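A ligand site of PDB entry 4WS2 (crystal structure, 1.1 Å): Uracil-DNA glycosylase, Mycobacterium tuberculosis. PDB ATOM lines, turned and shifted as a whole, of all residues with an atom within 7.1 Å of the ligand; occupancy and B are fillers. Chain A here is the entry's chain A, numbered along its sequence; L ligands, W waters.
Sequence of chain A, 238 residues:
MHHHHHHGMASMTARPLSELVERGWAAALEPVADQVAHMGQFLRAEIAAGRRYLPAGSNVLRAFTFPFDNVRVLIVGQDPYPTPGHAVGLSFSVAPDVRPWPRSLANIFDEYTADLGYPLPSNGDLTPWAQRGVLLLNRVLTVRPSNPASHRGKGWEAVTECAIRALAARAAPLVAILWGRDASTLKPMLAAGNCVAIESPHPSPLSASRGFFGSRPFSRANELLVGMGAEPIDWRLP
Gly 77 touches the ligand. Pro 80 touches the ligand. Tyr 81 touches the ligand (CD1 to N3, 3.3 Å). CA of Ser 91 touches O2 of the ligand, 3.4 Å away. Ser 104 touches the ligand (OG to N3, 3.7 Å). Hydrophobic or aromatic side chains that line the ligand: Tyr 81, Phe 92 and His 202. Within 4 Å of the ligand: Gly 77, Gln 78, Asp 79, Pro 80, Tyr 81, Ser 91, Phe 92, Ser 104, Asn 138 and His 202.
Water W2 bridges O2 of the ligand (2.7 Å) and N of Tyr 81 (3.0 Å).
OD1 of Asn 138 is in hydrogen-bond range of N1 of the ligand (2.9 Å). O2 of the ligand is in hydrogen-bond range of N of Phe 92 (2.9 Å). An oxygen (O1) of the ligand lies within hydrogen-bond range of the backbone NH (N) of Gln 78 (2.7 Å). An oxygen (O1) of the ligand sits at hydrogen-bond distance from a ring nitrogen (NE2) of His 202 (2.8 Å). The backbone carbonyl oxygen of Asp 79 is in hydrogen-bond range of a nitrogen (N1) of the ligand.
O of Gly 77 lies within hydrogen-bond range of N of Arg 139 (2.9 Å). N of Gln 78 sits at hydrogen-bond distance from OD1 of Asn 138 (3.4 Å). O of Leu 136 lies within hydrogen-bond range of N of Ser 91, 2.9 Å away. A ring nitrogen (ND1) of His 202 sits at hydrogen-bond distance from the backbone NH of Ser 204, at 3.0 Å. O of Leu 137 lies within hydrogen-bond range of N of Gly 77, at 3.0 Å. The side-chain hydroxyl (OH) of Tyr 81 is in hydrogen-bond range of the backbone carbonyl oxygen (O) of Phe 92 (2.7 Å). N of Arg 139 lies within hydrogen-bond range of O of Gln 78, 3.4 Å away. O of Gln 78 sits at hydrogen-bond distance from N of Val 140 (3.1 Å).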
ATOM      1  N   VAL A  76      23.150 -12.548  13.162  1.00  0.00           N
ATOM      2  CA  VAL A  76      24.564 -12.770  13.398  1.00  0.00           C
ATOM      3  C   VAL A  76      25.117 -11.718  14.347  1.00  0.00           C
ATOM      4  O   VAL A  76      24.989 -10.506  14.095  1.00  0.00           O
ATOM      5  CB  VAL A  76      25.388 -12.743  12.075  1.00  0.00           C
ATOM      6  CG1 VAL A  76      26.799 -13.208  12.354  1.00  0.00           C
ATOM      7  CG2 VAL A  76      24.726 -13.568  10.993  1.00  0.00           C
ATOM      8  N   GLY A  77      25.738 -12.204  15.430  1.00  0.00           N
ATOM      9  CA  GLY A  77      26.529 -11.373  16.274  1.00  0.00           C
ATOM     10  C   GLY A  77      28.019 -11.581  16.104  1.00  0.00           C
ATOM     11  O   GLY A  77      28.483 -12.056  15.055  1.00  0.00           O
ATOM     12  N   GLN A  78      28.771 -11.172  17.126  1.00  0.00           N
ATOM     13  CA  GLN A  78      30.219 -11.174  17.092  1.00  0.00           C
ATOM     14  C   GLN A  78      30.820 -12.490  17.535  1.00  0.00           C
ATOM     15  O   GLN A  78      31.538 -13.163  16.772  1.00  0.00           O
ATOM     16  CB  GLN A  78      30.739 -10.025  17.975  1.00  0.00           C
ATOM     17  CG  GLN A  78      32.252  -9.966  18.049  1.00  0.00           C
ATOM     18  CD  GLN A  78      32.767  -8.883  18.936  1.00  0.00           C
ATOM     19  OE1 GLN A  78      33.096  -9.118  20.145  1.00  0.00           O
ATOM     20  NE2 GLN A  78      32.810  -7.702  18.423  1.00  0.00           N
ATOM     21  N   ASP A  79      30.568 -12.853  18.789  1.00  0.00           N
ATOM     22  CA  ASP A  79      31.185 -14.025  19.403  1.00  0.00           C
ATOM     23  C   ASP A  79      30.388 -14.309  20.677  1.00  0.00           C
ATOM     24  O   ASP A  79      29.552 -13.499  21.077  1.00  0.00           O
ATOM     25  CB  ASP A  79      32.702 -13.849  19.632  1.00  0.00           C
ATOM     26  CG  ASP A  79      33.108 -12.844  20.715  1.00  0.00           C
ATOM     27  OD1 ASP A  79      32.380 -11.871  20.957  1.00  0.00           O
ATOM     28  OD2 ASP A  79      34.206 -13.054  21.290  1.00  0.00           O
ATOM     29  N   PRO A  80      30.615 -15.477  21.319  1.00  0.00           N
ATOM     30  CA  PRO A  80      29.734 -15.845  22.444  1.00  0.00           C
ATOM     31  C   PRO A  80      29.919 -14.995  23.683  1.00  0.00           C
ATOM     32  O   PRO A  80      30.941 -14.336  23.896  1.00  0.00           O
ATOM     33  CB  PRO A  80      30.128 -17.296  22.738  1.00  0.00           C
ATOM     34  CG  PRO A  80      30.681 -17.789  21.422  1.00  0.00           C
ATOM     35  CD  PRO A  80      31.452 -16.590  20.910  1.00  0.00           C
ATOM     36  N   TYR A  81      28.940 -15.090  24.581  1.00  0.00           N
ATOM     37  CA  TYR A  81      29.076 -14.438  25.871  1.00  0.00           C
ATOM     38  C   TYR A  81      30.361 -14.882  26.534  1.00  0.00           C
ATOM     39  O   TYR A  81      30.678 -16.079  26.564  1.00  0.00           O
ATOM     40  CB  TYR A  81      27.935 -14.798  26.824  1.00  0.00           C
ATOM     41  CG  TYR A  81      26.601 -14.187  26.460  1.00  0.00           C
ATOM     42  CD1 TYR A  81      26.402 -12.819  26.574  1.00  0.00           C
ATOM     43  CD2 TYR A  81      25.535 -14.961  26.023  1.00  0.00           C
ATOM     44  CE1 TYR A  81      25.188 -12.241  26.237  1.00  0.00           C
ATOM     45  CE2 TYR A  81      24.301 -14.407  25.697  1.00  0.00           C
ATOM     46  CZ  TYR A  81      24.136 -13.032  25.791  1.00  0.00           C
ATOM     47  OH  TYR A  81      22.964 -12.413  25.447  1.00  0.00           O
ATOM     48  N   PRO A  82      31.089 -13.942  27.193  1.00  0.00           N
ATOM     49  CA  PRO A  82      32.338 -14.312  27.804  1.00  0.00           C
ATOM     50  C   PRO A  82      32.251 -14.824  29.244  1.00  0.00           C
ATOM     51  O   PRO A  82      33.255 -15.258  29.795  1.00  0.00           O
ATOM     52  CB  PRO A  82      33.089 -12.977  27.784  1.00  0.00           C
ATOM     53  CG  PRO A  82      32.005 -11.931  27.985  1.00  0.00           C
ATOM     54  CD  PRO A  82      30.904 -12.477  27.106  1.00  0.00           C
ATOM     55  N   ALA A  87      26.935 -18.485  27.629  1.00  0.00           N
ATOM     56  CA  ALA A  87      26.807 -18.931  26.239  1.00  0.00           C
ATOM     57  C   ALA A  87      26.311 -20.352  26.142  1.00  0.00           C
ATOM     58  O   ALA A  87      26.776 -21.229  26.865  1.00  0.00           O
ATOM     59  CB  ALA A  87      28.142 -18.846  25.531  1.00  0.00           C
ATOM     60  N   VAL A  88      25.396 -20.570  25.195  1.00  0.00           N
ATOM     61  CA  VAL A  88      24.780 -21.889  24.994  1.00  0.00           C
ATOM     62  C   VAL A  88      24.893 -22.352  23.552  1.00  0.00           C
ATOM     63  O   VAL A  88      24.310 -23.388  23.194  1.00  0.00           O
ATOM     64  CB  VAL A  88      23.308 -21.906  25.463  1.00  0.00           C
ATOM     65  CG1 VAL A  88      23.219 -21.544  26.940  1.00  0.00           C
ATOM     66  CG2 VAL A  88      22.429 -21.038  24.587  1.00  0.00           C
ATOM     67  N   LEU A  90      23.748 -20.753  20.872  1.00  0.00           N
ATOM     68  CA  LEU A  90      22.810 -19.994  20.076  1.00  0.00           C
ATOM     69  C   LEU A  90      23.102 -18.542  20.424  1.00  0.00           C
ATOM     70  O   LEU A  90      23.075 -18.175  21.595  1.00  0.00           O
ATOM     71  CB  LEU A  90      21.367 -20.352  20.406  1.00  0.00           C
ATOM     72  CG  LEU A  90      20.972 -21.790  20.109  1.00  0.00           C
ATOM     73  CD1 LEU A  90      19.571 -22.098  20.616  1.00  0.00           C
ATOM     74  CD2 LEU A  90      21.112 -22.115  18.636  1.00  0.00           C
ATOM     75  N   SER A  91      23.426 -17.722  19.430  1.00  0.00           N
ATOM     76  CA  SER A  91      23.837 -16.374  19.722  1.00  0.00           C
ATOM     77  C   SER A  91      22.781 -15.647  20.560  1.00  0.00           C
ATOM     78  O   SER A  91      21.569 -15.777  20.350  1.00  0.00           O
ATOM     79  CB  SER A  91      24.238 -15.611  18.488  1.00  0.00           C
ATOM     80  OG  SER A  91      23.133 -15.416  17.626  1.00  0.00           O
ATOM     81  N   PHE A  92      23.298 -14.932  21.574  1.00  0.00           N
ATOM     82  CA  PHE A  92      22.531 -14.057  22.479  1.00  0.00           C
ATOM     83  C   PHE A  92      21.656 -14.789  23.490  1.00  0.00           C
ATOM     84  O   PHE A  92      21.253 -14.187  24.472  1.00  0.00           O
ATOM     85  CB  PHE A  92      21.745 -13.003  21.725  1.00  0.00           C
ATOM     86  CG  PHE A  92      22.638 -12.116  20.878  1.00  0.00           C
ATOM     87  CD1 PHE A  92      23.382 -11.119  21.471  1.00  0.00           C
ATOM     88  CD2 PHE A  92      22.759 -12.322  19.531  1.00  0.00           C
ATOM     89  CE1 PHE A  92      24.232 -10.317  20.706  1.00  0.00           C
ATOM     90  CE2 PHE A  92      23.630 -11.545  18.758  1.00  0.00           C
ATOM     91  CZ  PHE A  92      24.343 -10.556  19.358  1.00  0.00           C
ATOM     92  N   SER A  93      21.415 -16.067  23.290  1.00  0.00           N
ATOM     93  CA  SER A  93      20.528 -16.817  24.167  1.00  0.00           C
ATOM     94  C   SER A  93      21.207 -17.192  25.470  1.00  0.00           C
ATOM     95  O   SER A  93      22.413 -17.373  25.516  1.00  0.00           O
ATOM     96  CB  SER A  93      20.080 -18.090  23.435  1.00  0.00           C
ATOM     97  OG  SER A  93      18.952 -18.701  24.056  1.00  0.00           O
ATOM     98  N   PRO A 102      22.346 -10.942  30.691  1.00  0.00           N
ATOM     99  CA  PRO A 102      23.436 -10.151  30.195  1.00  0.00           C
ATOM    100  C   PRO A 102      22.955  -8.894  29.531  1.00  0.00           C
ATOM    101  O   PRO A 102      21.844  -8.832  28.999  1.00  0.00           O
ATOM    102  CB  PRO A 102      24.117 -11.038  29.188  1.00  0.00           C
ATOM    103  CG  PRO A 102      23.445 -12.313  29.174  1.00  0.00           C
ATOM    104  CD  PRO A 102      22.314 -12.292  30.112  1.00  0.00           C
ATOM    105  N   ARG A 103      23.819  -7.887  29.526  1.00  0.00           N
ATOM    106  CA  ARG A 103      23.434  -6.586  29.016  1.00  0.00           C
ATOM    107  C   ARG A 103      23.031  -6.570  27.545  1.00  0.00           C
ATOM    108  O   ARG A 103      22.051  -5.868  27.188  1.00  0.00           O
ATOM    109  CB  ARG A 103      24.507  -5.563  29.329  1.00  0.00           C
ATOM    110  CG  ARG A 103      24.634  -5.265  30.831  1.00  0.00           C
ATOM    111  CD  ARG A 103      25.809  -4.298  31.130  1.00  0.00           C
ATOM    112  NE  ARG A 103      26.131  -4.074  32.534  1.00  0.00           N
ATOM    113  CZ  ARG A 103      26.893  -4.853  33.300  1.00  0.00           C
ATOM    114  NH1 ARG A 103      27.439  -5.987  32.837  1.00  0.00           N
ATOM    115  NH2 ARG A 103      27.105  -4.493  34.564  1.00  0.00           N
ATOM    116  N   SER A 104      23.702  -7.317  26.672  1.00  0.00           N
ATOM    117  CA  SER A 104      23.275  -7.325  25.277  1.00  0.00           C
ATOM    118  C   SER A 104      21.860  -7.829  25.155  1.00  0.00           C
ATOM    119  O   SER A 104      21.077  -7.315  24.343  1.00  0.00           O
ATOM    120  CB  SER A 104      24.183  -8.178  24.357  1.00  0.00           C
ATOM    121  OG  SER A 104      25.400  -7.578  24.039  1.00  0.00           O
ATOM    122  N   LEU A 105      21.535  -8.868  25.929  1.00  0.00           N
ATOM    123  CA  LEU A 105      20.211  -9.439  25.879  1.00  0.00           C
ATOM    124  C   LEU A 105      19.150  -8.516  26.418  1.00  0.00           C
ATOM    125  O   LEU A 105      18.068  -8.390  25.859  1.00  0.00           O
ATOM    126  CB  LEU A 105      20.179 -10.791  26.575  1.00  0.00           C
ATOM    127  CG  LEU A 105      18.916 -11.603  26.389  1.00  0.00           C
ATOM    128  CD1 LEU A 105      18.612 -11.856  24.918  1.00  0.00           C
ATOM    129  CD2 LEU A 105      19.035 -12.931  27.101  1.00  0.00           C
ATOM    130  N   LEU A 136      20.586 -18.467  14.916  1.00  0.00           N
ATOM    131  CA  LEU A 136      21.224 -17.595  15.907  1.00  0.00           C
ATOM    132  C   LEU A 136      22.736 -17.813  15.882  1.00  0.00           C
ATOM    133  O   LEU A 136      23.283 -18.620  16.651  1.00  0.00           O
ATOM    134  CB  LEU A 136      20.618 -17.852  17.288  1.00  0.00           C
ATOM    135  CG  LEU A 136      19.127 -17.522  17.399  1.00  0.00           C
ATOM    136  CD1 LEU A 136      18.517 -18.006  18.691  1.00  0.00           C
ATOM    137  CD2 LEU A 136      18.922 -16.032  17.270  1.00  0.00           C
ATOM    138  N   LEU A 137      23.362 -17.134  14.919  1.00  0.00           N
ATOM    139  CA  LEU A 137      24.775 -17.333  14.654  1.00  0.00           C
ATOM    140  C   LEU A 137      25.633 -16.222  15.277  1.00  0.00           C
ATOM    141  O   LEU A 137      25.159 -15.120  15.512  1.00  0.00           O
ATOM    142  CB  LEU A 137      24.997 -17.356  13.153  1.00  0.00           C
ATOM    143  CG  LEU A 137      26.264 -17.999  12.592  1.00  0.00           C
ATOM    144  CD1 LEU A 137      26.378 -19.454  13.018  1.00  0.00           C
ATOM    145  CD2 LEU A 137      26.274 -17.838  11.081  1.00  0.00           C
ATOM    146  N   ASN A 138      26.906 -16.532  15.517  1.00  0.00           N
ATOM    147  CA  ASN A 138      27.933 -15.552  15.739  1.00  0.00           C
ATOM    148  C   ASN A 138      28.993 -15.686  14.651  1.00  0.00           C
ATOM    149  O   ASN A 138      29.217 -16.775  14.137  1.00  0.00           O
ATOM    150  CB  ASN A 138      28.570 -15.721  17.129  1.00  0.00           C
ATOM    151  CG  ASN A 138      27.731 -15.149  18.232  1.00  0.00           C
ATOM    152  OD1 ASN A 138      27.269 -14.026  18.124  1.00  0.00           O
ATOM    153  ND2 ASN A 138      27.583 -15.907  19.320  1.00  0.00           N
ATOM    154  N   ARG A 139      29.680 -14.585  14.336  1.00  0.00           N
ATOM    155  CA  ARG A 139      30.721 -14.636  13.332  1.00  0.00           C
ATOM    156  C   ARG A 139      31.848 -15.587  13.729  1.00  0.00           C
ATOM    157  O   ARG A 139      32.432 -16.276  12.888  1.00  0.00           O
ATOM    158  CB  ARG A 139      31.258 -13.227  13.118  1.00  0.00           C
ATOM    159  CG  ARG A 139      32.181 -13.077  11.902  1.00  0.00           C
ATOM    160  CD  ARG A 139      31.419 -13.148  10.561  1.00  0.00           C
ATOM    161  NE  ARG A 139      32.264 -12.762   9.455  1.00  0.00           N
ATOM    162  CZ  ARG A 139      32.997 -13.586   8.699  1.00  0.00           C
ATOM    163  NH1 ARG A 139      32.886 -14.918   8.808  1.00  0.00           N
ATOM    164  NH2 ARG A 139      33.815 -13.080   7.798  1.00  0.00           N
ATOM    165  N   VAL A 140      32.154 -15.604  15.021  1.00  0.00           N
ATOM    166  CA  VAL A 140      33.131 -16.468  15.637  1.00  0.00           C
ATOM    167  C   VAL A 140      32.425 -17.287  16.720  1.00  0.00           C
ATOM    168  O   VAL A 140      31.623 -16.727  17.475  1.00  0.00           O
ATOM    169  CB  VAL A 140      34.304 -15.628  16.185  1.00  0.00           C
ATOM    170  CG1 VAL A 140      35.189 -16.373  17.136  1.00  0.00           C
ATOM    171  CG2 VAL A 140      35.053 -15.003  15.009  1.00  0.00           C
ATOM    172  N   TRP A 179      24.382  -7.780  13.389  1.00  0.00           N
ATOM    173  CA  TRP A 179      24.560  -6.921  14.538  1.00  0.00           C
ATOM    174  C   TRP A 179      26.028  -6.712  14.833  1.00  0.00           C
ATOM    175  O   TRP A 179      26.721  -7.621  15.332  1.00  0.00           O
ATOM    176  CB  TRP A 179      23.842  -7.496  15.771  1.00  0.00           C
ATOM    177  CG  TRP A 179      22.337  -7.310  15.749  1.00  0.00           C
ATOM    178  CD1 TRP A 179      21.622  -6.377  15.059  1.00  0.00           C
ATOM    179  CD2 TRP A 179      21.364  -8.054  16.500  1.00  0.00           C
ATOM    180  NE1 TRP A 179      20.291  -6.502  15.301  1.00  0.00           N
ATOM    181  CE2 TRP A 179      20.109  -7.524  16.184  1.00  0.00           C
ATOM    182  CE3 TRP A 179      21.456  -9.116  17.393  1.00  0.00           C
ATOM    183  CZ2 TRP A 179      18.932  -8.021  16.748  1.00  0.00           C
ATOM    184  CZ3 TRP A 179      20.304  -9.597  17.948  1.00  0.00           C
ATOM    185  CH2 TRP A 179      19.052  -9.062  17.603  1.00  0.00           C
ATOM    186  N   HIS A 202      25.700  -3.129  17.054  1.00  0.00           N
ATOM    187  CA  HIS A 202      25.516  -4.218  17.979  1.00  0.00           C
ATOM    188  C   HIS A 202      24.714  -3.751  19.202  1.00  0.00           C
ATOM    189  O   HIS A 202      24.815  -2.603  19.630  1.00  0.00           O
ATOM    190  CB  HIS A 202      26.917  -4.722  18.324  1.00  0.00           C
ATOM    191  CG  HIS A 202      26.977  -6.026  19.048  1.00  0.00           C
ATOM    192  ND1 HIS A 202      26.680  -6.139  20.377  1.00  0.00           N
ATOM    193  CD2 HIS A 202      27.345  -7.266  18.618  1.00  0.00           C
ATOM    194  CE1 HIS A 202      26.850  -7.392  20.746  1.00  0.00           C
ATOM    195  NE2 HIS A 202      27.239  -8.098  19.693  1.00  0.00           N
ATOM    196  N   PRO A 203      23.929  -4.668  19.779  1.00  0.00           N
ATOM    197  CA  PRO A 203      23.105  -4.309  20.938  1.00  0.00           C
ATOM    198  C   PRO A 203      23.875  -4.106  22.235  1.00  0.00           C
ATOM    199  O   PRO A 203      23.286  -3.680  23.195  1.00  0.00           O
ATOM    200  CB  PRO A 203      22.115  -5.446  21.028  1.00  0.00           C
ATOM    201  CG  PRO A 203      22.771  -6.599  20.376  1.00  0.00           C
ATOM    202  CD  PRO A 203      23.565  -6.002  19.257  1.00  0.00           C
ATOM    203  N   SER A 204      25.150  -4.442  22.265  1.00  0.00           N
ATOM    204  CA  SER A 204      25.935  -4.218  23.455  1.00  0.00           C
ATOM    205  C   SER A 204      25.829  -2.753  23.881  1.00  0.00           C
ATOM    206  O   SER A 204      25.786  -1.854  23.048  1.00  0.00           O
ATOM    207  CB  SER A 204      27.360  -4.597  23.190  1.00  0.00           C
ATOM    208  OG  SER A 204      28.257  -3.916  24.035  1.00  0.00           O
HETATM  209  O1  LIG L   1      27.758 -10.809  19.619  1.00  0.00           O
HETATM  210  C1  LIG L   1      27.381 -11.413  20.673  1.00  0.00           C
HETATM  211  N1  LIG L   1      26.840 -12.650  20.589  1.00  0.00           N
HETATM  212  C2  LIG L   1      26.483 -13.322  21.711  1.00  0.00           C
HETATM  213  O2  LIG L   1      26.125 -14.568  21.522  1.00  0.00           O
HETATM  214  N2  LIG L   1      27.498 -10.820  21.882  1.00  0.00           N
HETATM  215  C3  LIG L   1      27.123 -11.456  23.004  1.00  0.00           C
HETATM  216  N3  LIG L   1      27.286 -10.749  24.137  1.00  0.00           N
HETATM  217  C4  LIG L   1      26.599 -12.736  22.949  1.00  0.00           C
HETATM  218  O   HOH W   1      30.207  -9.897  21.894  1.00  0.00           O
HETATM  219  O   HOH W   2      26.668 -16.561  23.313  1.00  0.00           O
